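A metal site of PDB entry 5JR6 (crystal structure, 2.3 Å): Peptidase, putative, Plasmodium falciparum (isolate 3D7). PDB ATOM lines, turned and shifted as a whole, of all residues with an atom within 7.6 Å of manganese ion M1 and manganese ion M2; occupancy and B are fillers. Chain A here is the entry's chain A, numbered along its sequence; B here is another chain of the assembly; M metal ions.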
ATOM      1  N   PHE A 418      -3.865   0.616   5.508  1.00  0.00           N
ATOM      2  CA  PHE A 418      -5.027   0.803   4.676  1.00  0.00           C
ATOM      3  C   PHE A 418      -5.225   2.284   4.619  1.00  0.00           C
ATOM      4  O   PHE A 418      -4.580   3.009   5.361  1.00  0.00           O
ATOM      5  CB  PHE A 418      -6.301   0.087   5.228  1.00  0.00           C
ATOM      6  CG  PHE A 418      -6.674   0.492   6.635  1.00  0.00           C
ATOM      7  CD1 PHE A 418      -7.488   1.611   6.877  1.00  0.00           C
ATOM      8  CD2 PHE A 418      -6.224  -0.231   7.721  1.00  0.00           C
ATOM      9  CE1 PHE A 418      -7.843   1.978   8.178  1.00  0.00           C
ATOM     10  CE2 PHE A 418      -6.583   0.122   9.039  1.00  0.00           C
ATOM     11  CZ  PHE A 418      -7.396   1.242   9.259  1.00  0.00           C
ATOM     12  N   ILE A 421      -9.476   6.409   7.364  1.00  0.00           N
ATOM     13  CA  ILE A 421     -10.797   7.004   7.376  1.00  0.00           C
ATOM     14  C   ILE A 421     -10.804   8.133   8.394  1.00  0.00           C
ATOM     15  O   ILE A 421     -10.645   7.928   9.599  1.00  0.00           O
ATOM     16  CB  ILE A 421     -11.890   5.947   7.717  1.00  0.00           C
ATOM     17  CG1 ILE A 421     -11.842   4.830   6.689  1.00  0.00           C
ATOM     18  CG2 ILE A 421     -13.272   6.599   7.711  1.00  0.00           C
ATOM     19  CD1 ILE A 421     -12.584   3.574   7.094  1.00  0.00           C
ATOM     20  N   LEU A 450     -12.034   8.289  13.391  1.00  0.00           N
ATOM     21  CA  LEU A 450     -10.724   8.007  12.829  1.00  0.00           C
ATOM     22  C   LEU A 450     -10.463   6.503  12.854  1.00  0.00           C
ATOM     23  O   LEU A 450     -10.273   5.917  13.919  1.00  0.00           O
ATOM     24  CB  LEU A 450      -9.630   8.752  13.599  1.00  0.00           C
ATOM     25  CG  LEU A 450      -8.216   8.508  13.070  1.00  0.00           C
ATOM     26  CD1 LEU A 450      -8.017   9.290  11.781  1.00  0.00           C
ATOM     27  CD2 LEU A 450      -7.090   8.873  14.077  1.00  0.00           C
ATOM     28  N   ASP A 451     -10.424   5.898  11.676  1.00  0.00           N
ATOM     29  CA  ASP A 451     -10.126   4.491  11.514  1.00  0.00           C
ATOM     30  C   ASP A 451      -8.765   4.453  10.791  1.00  0.00           C
ATOM     31  O   ASP A 451      -8.647   4.926   9.663  1.00  0.00           O
ATOM     32  CB  ASP A 451     -11.227   3.798  10.708  1.00  0.00           C
ATOM     33  CG  ASP A 451     -11.128   2.281  10.722  1.00  0.00           C
ATOM     34  OD1 ASP A 451     -10.135   1.743  11.265  1.00  0.00           O
ATOM     35  OD2 ASP A 451     -12.069   1.610  10.210  1.00  0.00           O
ATOM     36  N   SER A 452      -7.735   3.963  11.451  1.00  0.00           N
ATOM     37  CA  SER A 452      -6.398   4.032  10.899  1.00  0.00           C
ATOM     38  C   SER A 452      -5.543   2.915  11.433  1.00  0.00           C
ATOM     39  O   SER A 452      -5.888   2.282  12.438  1.00  0.00           O
ATOM     40  CB  SER A 452      -5.751   5.382  11.210  1.00  0.00           C
ATOM     41  OG  SER A 452      -5.351   5.428  12.574  1.00  0.00           O
ATOM     42  N   GLY A 453      -4.437   2.648  10.740  1.00  0.00           N
ATOM     43  CA  GLY A 453      -3.574   1.530  11.113  1.00  0.00           C
ATOM     44  C   GLY A 453      -2.247   1.589  10.412  1.00  0.00           C
ATOM     45  O   GLY A 453      -2.057   2.366   9.482  1.00  0.00           O
ATOM     46  N   THR A 461      -1.544  -3.235  12.343  1.00  0.00           N
ATOM     47  CA  THR A 461      -2.509  -2.691  13.312  1.00  0.00           C
ATOM     48  C   THR A 461      -3.719  -2.076  12.625  1.00  0.00           C
ATOM     49  O   THR A 461      -3.628  -1.607  11.481  1.00  0.00           O
ATOM     50  CB  THR A 461      -1.888  -1.616  14.213  1.00  0.00           C
ATOM     51  OG1 THR A 461      -1.688  -0.410  13.459  1.00  0.00           O
ATOM     52  CG2 THR A 461      -0.552  -2.092  14.762  1.00  0.00           C
ATOM     53  N   ASP A 462      -4.860  -2.155  13.294  1.00  0.00           N
ATOM     54  CA  ASP A 462      -6.103  -1.563  12.841  1.00  0.00           C
ATOM     55  C   ASP A 462      -6.901  -1.042  14.037  1.00  0.00           C
ATOM     56  O   ASP A 462      -7.328  -1.833  14.868  1.00  0.00           O
ATOM     57  CB  ASP A 462      -6.891  -2.627  12.087  1.00  0.00           C
ATOM     58  CG  ASP A 462      -8.126  -2.107  11.418  1.00  0.00           C
ATOM     59  OD1 ASP A 462      -8.714  -2.903  10.675  1.00  0.00           O
ATOM     60  OD2 ASP A 462      -8.525  -0.932  11.610  1.00  0.00           O
ATOM     61  N   VAL A 463      -7.184   0.256  14.117  1.00  0.00           N
ATOM     62  CA  VAL A 463      -7.813   0.806  15.320  1.00  0.00           C
ATOM     63  C   VAL A 463      -8.770   1.926  14.942  1.00  0.00           C
ATOM     64  O   VAL A 463      -8.442   2.764  14.093  1.00  0.00           O
ATOM     65  CB  VAL A 463      -6.761   1.349  16.338  1.00  0.00           C
ATOM     66  CG1 VAL A 463      -5.754   2.287  15.645  1.00  0.00           C
ATOM     67  CG2 VAL A 463      -7.459   2.091  17.512  1.00  0.00           C
ATOM     68  N   THR A 464      -9.953   1.949  15.546  1.00  0.00           N
ATOM     69  CA  THR A 464     -10.844   3.092  15.400  1.00  0.00           C
ATOM     70  C   THR A 464     -11.208   3.687  16.750  1.00  0.00           C
ATOM     71  O   THR A 464     -11.417   2.970  17.734  1.00  0.00           O
ATOM     72  CB  THR A 464     -12.148   2.735  14.650  1.00  0.00           C
ATOM     73  OG1 THR A 464     -11.836   1.965  13.480  1.00  0.00           O
ATOM     74  CG2 THR A 464     -12.907   3.993  14.244  1.00  0.00           C
ATOM     75  N   GLY A 522     -19.499  -6.820   9.650  1.00  0.00           N
ATOM     76  CA  GLY A 522     -19.076  -7.806  10.633  1.00  0.00           C
ATOM     77  C   GLY A 522     -18.422  -7.153  11.841  1.00  0.00           C
ATOM     78  O   GLY A 522     -18.061  -5.970  11.795  1.00  0.00           O
ATOM     79  N   THR A 523     -18.331  -7.888  12.938  1.00  0.00           N
ATOM     80  CA  THR A 523     -17.749  -7.358  14.177  1.00  0.00           C
ATOM     81  C   THR A 523     -16.227  -7.462  14.254  1.00  0.00           C
ATOM     82  O   THR A 523     -15.561  -6.613  14.866  1.00  0.00           O
ATOM     83  CB  THR A 523     -18.357  -8.081  15.411  1.00  0.00           C
ATOM     84  OG1 THR A 523     -19.779  -7.856  15.436  1.00  0.00           O
ATOM     85  CG2 THR A 523     -17.744  -7.577  16.706  1.00  0.00           C
ATOM     86  N   GLY A 524     -15.676  -8.525  13.683  1.00  0.00           N
ATOM     87  CA  GLY A 524     -14.235  -8.702  13.706  1.00  0.00           C
ATOM     88  C   GLY A 524     -13.719  -9.571  12.584  1.00  0.00           C
ATOM     89  O   GLY A 524     -14.440 -10.449  12.074  1.00  0.00           O
ATOM     90  N   HIS A 525     -12.468  -9.338  12.221  1.00  0.00           N
ATOM     91  CA  HIS A 525     -11.743 -10.115  11.228  1.00  0.00           C
ATOM     92  C   HIS A 525     -10.393 -10.513  11.807  1.00  0.00           C
ATOM     93  O   HIS A 525      -9.877  -9.858  12.729  1.00  0.00           O
ATOM     94  CB  HIS A 525     -11.559  -9.307   9.938  1.00  0.00           C
ATOM     95  CG  HIS A 525     -10.957  -7.951  10.156  1.00  0.00           C
ATOM     96  ND1 HIS A 525      -9.611  -7.759  10.398  1.00  0.00           N
ATOM     97  CD2 HIS A 525     -11.511  -6.710  10.165  1.00  0.00           C
ATOM     98  CE1 HIS A 525      -9.363  -6.462  10.546  1.00  0.00           C
ATOM     99  NE2 HIS A 525     -10.498  -5.809  10.406  1.00  0.00           N
ATOM    100  N   GLY A 526      -9.800 -11.574  11.272  1.00  0.00           N
ATOM    101  CA  GLY A 526      -8.432 -11.922  11.594  1.00  0.00           C
ATOM    102  C   GLY A 526      -7.498 -10.861  11.014  1.00  0.00           C
ATOM    103  O   GLY A 526      -7.912 -10.064  10.158  1.00  0.00           O
ATOM    104  N   VAL A 527      -6.254 -10.814  11.499  1.00  0.00           N
ATOM    105  CA  VAL A 527      -5.303  -9.796  11.081  1.00  0.00           C
ATOM    106  C   VAL A 527      -3.916 -10.391  10.941  1.00  0.00           C
ATOM    107  O   VAL A 527      -3.457 -11.127  11.816  1.00  0.00           O
ATOM    108  CB  VAL A 527      -5.278  -8.602  12.077  1.00  0.00           C
ATOM    109  CG1 VAL A 527      -4.172  -7.584  11.732  1.00  0.00           C
ATOM    110  CG2 VAL A 527      -6.629  -7.920  12.097  1.00  0.00           C
ATOM    111  N   VAL A 533      -4.428  -6.349   6.404  1.00  0.00           N
ATOM    112  CA  VAL A 533      -5.169  -5.946   7.562  1.00  0.00           C
ATOM    113  C   VAL A 533      -6.410  -6.829   7.695  1.00  0.00           C
ATOM    114  O   VAL A 533      -6.895  -7.044   8.790  1.00  0.00           O
ATOM    115  CB  VAL A 533      -5.560  -4.462   7.483  1.00  0.00           C
ATOM    116  CG1 VAL A 533      -6.596  -4.234   6.367  1.00  0.00           C
ATOM    117  CG2 VAL A 533      -6.072  -3.977   8.826  1.00  0.00           C
ATOM    118  N   HIS A 534      -6.895  -7.369   6.577  1.00  0.00           N
ATOM    119  CA  HIS A 534      -7.987  -8.354   6.610  1.00  0.00           C
ATOM    120  C   HIS A 534      -7.455  -9.723   6.246  1.00  0.00           C
ATOM    121  O   HIS A 534      -7.134  -9.989   5.097  1.00  0.00           O
ATOM    122  CB  HIS A 534      -9.106  -7.961   5.661  1.00  0.00           C
ATOM    123  CG  HIS A 534      -9.823  -6.721   6.085  1.00  0.00           C
ATOM    124  ND1 HIS A 534     -10.352  -5.818   5.185  1.00  0.00           N
ATOM    125  CD2 HIS A 534     -10.076  -6.204   7.309  1.00  0.00           C
ATOM    126  CE1 HIS A 534     -10.903  -4.822   5.831  1.00  0.00           C
ATOM    127  NE2 HIS A 534     -10.745  -5.025   7.130  1.00  0.00           N
ATOM    128  N   SER A 555     -10.001  -8.365  15.331  1.00  0.00           N
ATOM    129  CA  SER A 555     -10.533  -7.046  15.585  1.00  0.00           C
ATOM    130  C   SER A 555     -11.863  -7.174  16.348  1.00  0.00           C
ATOM    131  O   SER A 555     -12.499  -8.229  16.363  1.00  0.00           O
ATOM    132  CB  SER A 555     -10.723  -6.248  14.288  1.00  0.00           C
ATOM    133  OG  SER A 555     -11.693  -6.796  13.407  1.00  0.00           O
ATOM    134  N   ASN A 556     -12.193  -6.115  17.074  1.00  0.00           N
ATOM    135  CA  ASN A 556     -13.447  -5.992  17.787  1.00  0.00           C
ATOM    136  C   ASN A 556     -13.967  -4.627  17.437  1.00  0.00           C
ATOM    137  O   ASN A 556     -13.462  -3.642  17.965  1.00  0.00           O
ATOM    138  CB  ASN A 556     -13.129  -6.154  19.268  1.00  0.00           C
ATOM    139  CG  ASN A 556     -14.240  -5.743  20.189  1.00  0.00           C
ATOM    140  OD1 ASN A 556     -15.374  -5.445  19.794  1.00  0.00           O
ATOM    141  ND2 ASN A 556     -13.920  -5.759  21.468  1.00  0.00           N
ATOM    142  N   GLU A 557     -14.962  -4.541  16.573  1.00  0.00           N
ATOM    143  CA  GLU A 557     -15.300  -3.225  16.051  1.00  0.00           C
ATOM    144  C   GLU A 557     -16.784  -3.000  15.783  1.00  0.00           C
ATOM    145  O   GLU A 557     -17.169  -2.751  14.643  1.00  0.00           O
ATOM    146  CB  GLU A 557     -14.503  -2.938  14.771  1.00  0.00           C
ATOM    147  CG  GLU A 557     -14.553  -4.044  13.716  1.00  0.00           C
ATOM    148  CD  GLU A 557     -13.587  -3.793  12.554  1.00  0.00           C
ATOM    149  OE1 GLU A 557     -13.505  -2.637  12.063  1.00  0.00           O
ATOM    150  OE2 GLU A 557     -12.877  -4.758  12.158  1.00  0.00           O
ATOM    151  N   ARG A 569     -17.793   4.213  15.554  1.00  0.00           N
ATOM    152  CA  ARG A 569     -17.240   2.868  15.539  1.00  0.00           C
ATOM    153  C   ARG A 569     -16.127   2.855  16.559  1.00  0.00           C
ATOM    154  O   ARG A 569     -15.443   3.853  16.754  1.00  0.00           O
ATOM    155  CB  ARG A 569     -16.748   2.474  14.129  1.00  0.00           C
ATOM    156  CG  ARG A 569     -16.017   1.102  14.062  1.00  0.00           C
ATOM    157  CD  ARG A 569     -15.875   0.549  12.603  1.00  0.00           C
ATOM    158  NE  ARG A 569     -15.048   1.399  11.738  1.00  0.00           N
ATOM    159  CZ  ARG A 569     -15.538   2.231  10.826  1.00  0.00           C
ATOM    160  NH1 ARG A 569     -16.853   2.326  10.661  1.00  0.00           N
ATOM    161  NH2 ARG A 569     -14.719   2.976  10.080  1.00  0.00           N
ATOM    162  N   GLU A 571     -12.953   0.334  17.749  1.00  0.00           N
ATOM    163  CA  GLU A 571     -12.269  -0.856  17.310  1.00  0.00           C
ATOM    164  C   GLU A 571     -10.957  -1.087  18.011  1.00  0.00           C
ATOM    165  O   GLU A 571     -10.114  -0.197  18.096  1.00  0.00           O
ATOM    166  CB  GLU A 571     -12.009  -0.786  15.812  1.00  0.00           C
ATOM    167  CG  GLU A 571     -11.103  -1.871  15.301  1.00  0.00           C
ATOM    168  CD  GLU A 571     -10.782  -1.672  13.840  1.00  0.00           C
ATOM    169  OE1 GLU A 571     -10.939  -0.528  13.344  1.00  0.00           O
ATOM    170  OE2 GLU A 571     -10.409  -2.668  13.191  1.00  0.00           O
ATOM    171  N   ASN A 572     -10.799  -2.300  18.523  1.00  0.00           N
ATOM    172  CA  ASN A 572      -9.527  -2.768  19.040  1.00  0.00           C
ATOM    173  C   ASN A 572      -9.142  -4.014  18.301  1.00  0.00           C
ATOM    174  O   ASN A 572      -9.970  -4.658  17.648  1.00  0.00           O
ATOM    175  CB  ASN A 572      -9.591  -3.106  20.531  1.00  0.00           C
ATOM    176  CG  ASN A 572      -9.587  -1.893  21.427  1.00  0.00           C
ATOM    177  OD1 ASN A 572      -9.772  -0.753  20.973  1.00  0.00           O
ATOM    178  ND2 ASN A 572      -9.376  -2.134  22.721  1.00  0.00           N
ATOM    179  N   MET A 573      -7.861  -4.362  18.422  1.00  0.00           N
ATOM    180  CA  MET A 573      -7.412  -5.697  18.105  1.00  0.00           C
ATOM    181  C   MET A 573      -7.038  -6.352  19.427  1.00  0.00           C
ATOM    182  O   MET A 573      -6.584  -5.687  20.352  1.00  0.00           O
ATOM    183  CB  MET A 573      -6.202  -5.681  17.126  1.00  0.00           C
ATOM    184  CG  MET A 573      -6.615  -5.458  15.669  1.00  0.00           C
ATOM    185  SD  MET A 573      -5.145  -5.038  14.620  1.00  0.00           S
ATOM    186  CE  MET A 573      -4.109  -6.425  15.000  1.00  0.00           C
ATOM    187  CB  01B B   1     -10.741  -1.449   7.640  1.00  0.00           C
ATOM    188  CA  01B B   1     -11.901  -1.310   8.573  1.00  0.00           C
ATOM    189  N   01B B   1      -9.632  -0.895   8.304  1.00  0.00           N
ATOM    190  O2  01B B   1     -11.403  -1.128   9.877  1.00  0.00           O
ATOM    191  C   01B B   1     -12.711  -2.560   8.590  1.00  0.00           C
ATOM    192  C6  01B B   1     -11.052  -0.639   6.385  1.00  0.00           C
ATOM    193  C7  01B B   1     -10.318  -1.234   5.132  1.00  0.00           C
ATOM    194  C8  01B B   1      -9.247  -2.040   5.299  1.00  0.00           C
ATOM    195  C9  01B B   1      -8.517  -2.625   4.082  1.00  0.00           C
ATOM    196  C10 01B B   1      -8.956  -2.330   2.808  1.00  0.00           C
ATOM    197  C11 01B B   1     -10.155  -1.427   2.623  1.00  0.00           C
ATOM    198  C12 01B B   1     -10.807  -0.905   3.711  1.00  0.00           C
ATOM    199  O   01B B   1     -12.157  -3.641   8.486  1.00  0.00           O
ATOM    200  N   PRO B   2     -14.157  -2.438   8.772  1.00  0.00           N
ATOM    201  CA  PRO B   2     -15.136  -3.530   8.835  1.00  0.00           C
ATOM    202  C   PRO B   2     -14.925  -4.641   7.899  1.00  0.00           C
ATOM    203  O   PRO B   2     -14.625  -4.422   6.715  1.00  0.00           O
ATOM    204  CB  PRO B   2     -16.445  -2.833   8.518  1.00  0.00           C
ATOM    205  CG  PRO B   2     -16.285  -1.450   9.018  1.00  0.00           C
ATOM    206  CD  PRO B   2     -14.815  -1.184   8.915  1.00  0.00           C
ATOM    207  N   PRO B   3     -15.114  -6.046   8.388  1.00  0.00           N
ATOM    208  CA  PRO B   3     -14.962  -7.246   7.570  1.00  0.00           C
ATOM    209  C   PRO B   3     -16.050  -7.278   6.516  1.00  0.00           C
ATOM    210  O   PRO B   3     -15.825  -7.772   5.425  1.00  0.00           O
ATOM    211  CB  PRO B   3     -15.055  -8.406   8.537  1.00  0.00           C
ATOM    212  CG  PRO B   3     -15.543  -7.839   9.834  1.00  0.00           C
ATOM    213  CD  PRO B   3     -15.482  -6.392   9.734  1.00  0.00           C
HETATM  214 MN    MN M   1     -10.329  -0.226  11.247  1.00  0.00          MN
HETATM  215 MN    MN M   2     -10.954  -3.529  11.040  1.00  0.00          MN
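Manganese ion M1 is bound by O2 of 01B 1 of chain B (2.0 Å), OD2 of Asp 462 (2.0 Å), OD1 of Asp 451 (2.0 Å) and OE1 of Glu 571 (2.2 Å).
Slightly farther from manganese ion M1 lies OD2 of Asp 451 (2.7 Å).
Merely in contact with manganese ion M1: Thr 464 (3.5 Å) and Phe 418 (3.8 Å).
Within 4 Å of manganese ion M1: Phe 418, Asp 451, Asp 462, Thr 464, Glu 571 and 01B 1 of chain B.
A ring nitrogen (NE2) of His 525 sits close to O of 01B 1 of chain B (3.3 Å).
The side-chain sulfur of Met 573 lies within hydrogen-bond range of the backbone NH of Asp 462 (3.2 Å).
The side-chain hydroxyl of Thr 464 lies close to the side-chain carboxylate of Asp 451 (3.3 Å).
NH2 of Arg 569 is in salt-bridge range of OD2 of Asp 451 (3.0 Å).
N of Glu 571 sits at hydrogen-bond distance from O of Thr 464 (3.1 Å).
NE2 of His 525 sits close to NE2 of His 534, at 3.4 Å.
The side-chain carboxylate (OE2) of Glu 557 sits close to the side-chain hydroxyl (OG) of Ser 555, at 2.7 Å.
The backbone NH (N) of Glu 557 lies within hydrogen-bond range of the backbone carbonyl oxygen (O) of Thr 523 (2.8 Å).
Within 4 Å of manganese ion M2: Asp 462, His 525, Glu 557, Glu 571 and 01B 1 of chain B.
OD1 of Asp 462 is bound to manganese ion M2 (2.4 Å).
Manganese ion M2 is bound by OE2 of Glu 571, 2.4 Å away.
Manganese ion M2 is bound by NE2 of His 525, 2.4 Å away.
Manganese ion M2 is bound by the side-chain carboxylate (OE2) of Glu 557 (2.5 Å).
Slightly farther from manganese ion M2 lies O2 of 01B 1 of chain B (2.7 Å).
Slightly farther from manganese ion M2 lies O of 01B 1 of chain B (2.8 Å).
Slightly farther from manganese ion M2 lies the side-chain carboxylate (OE1) of Glu 557 (2.9 Å).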
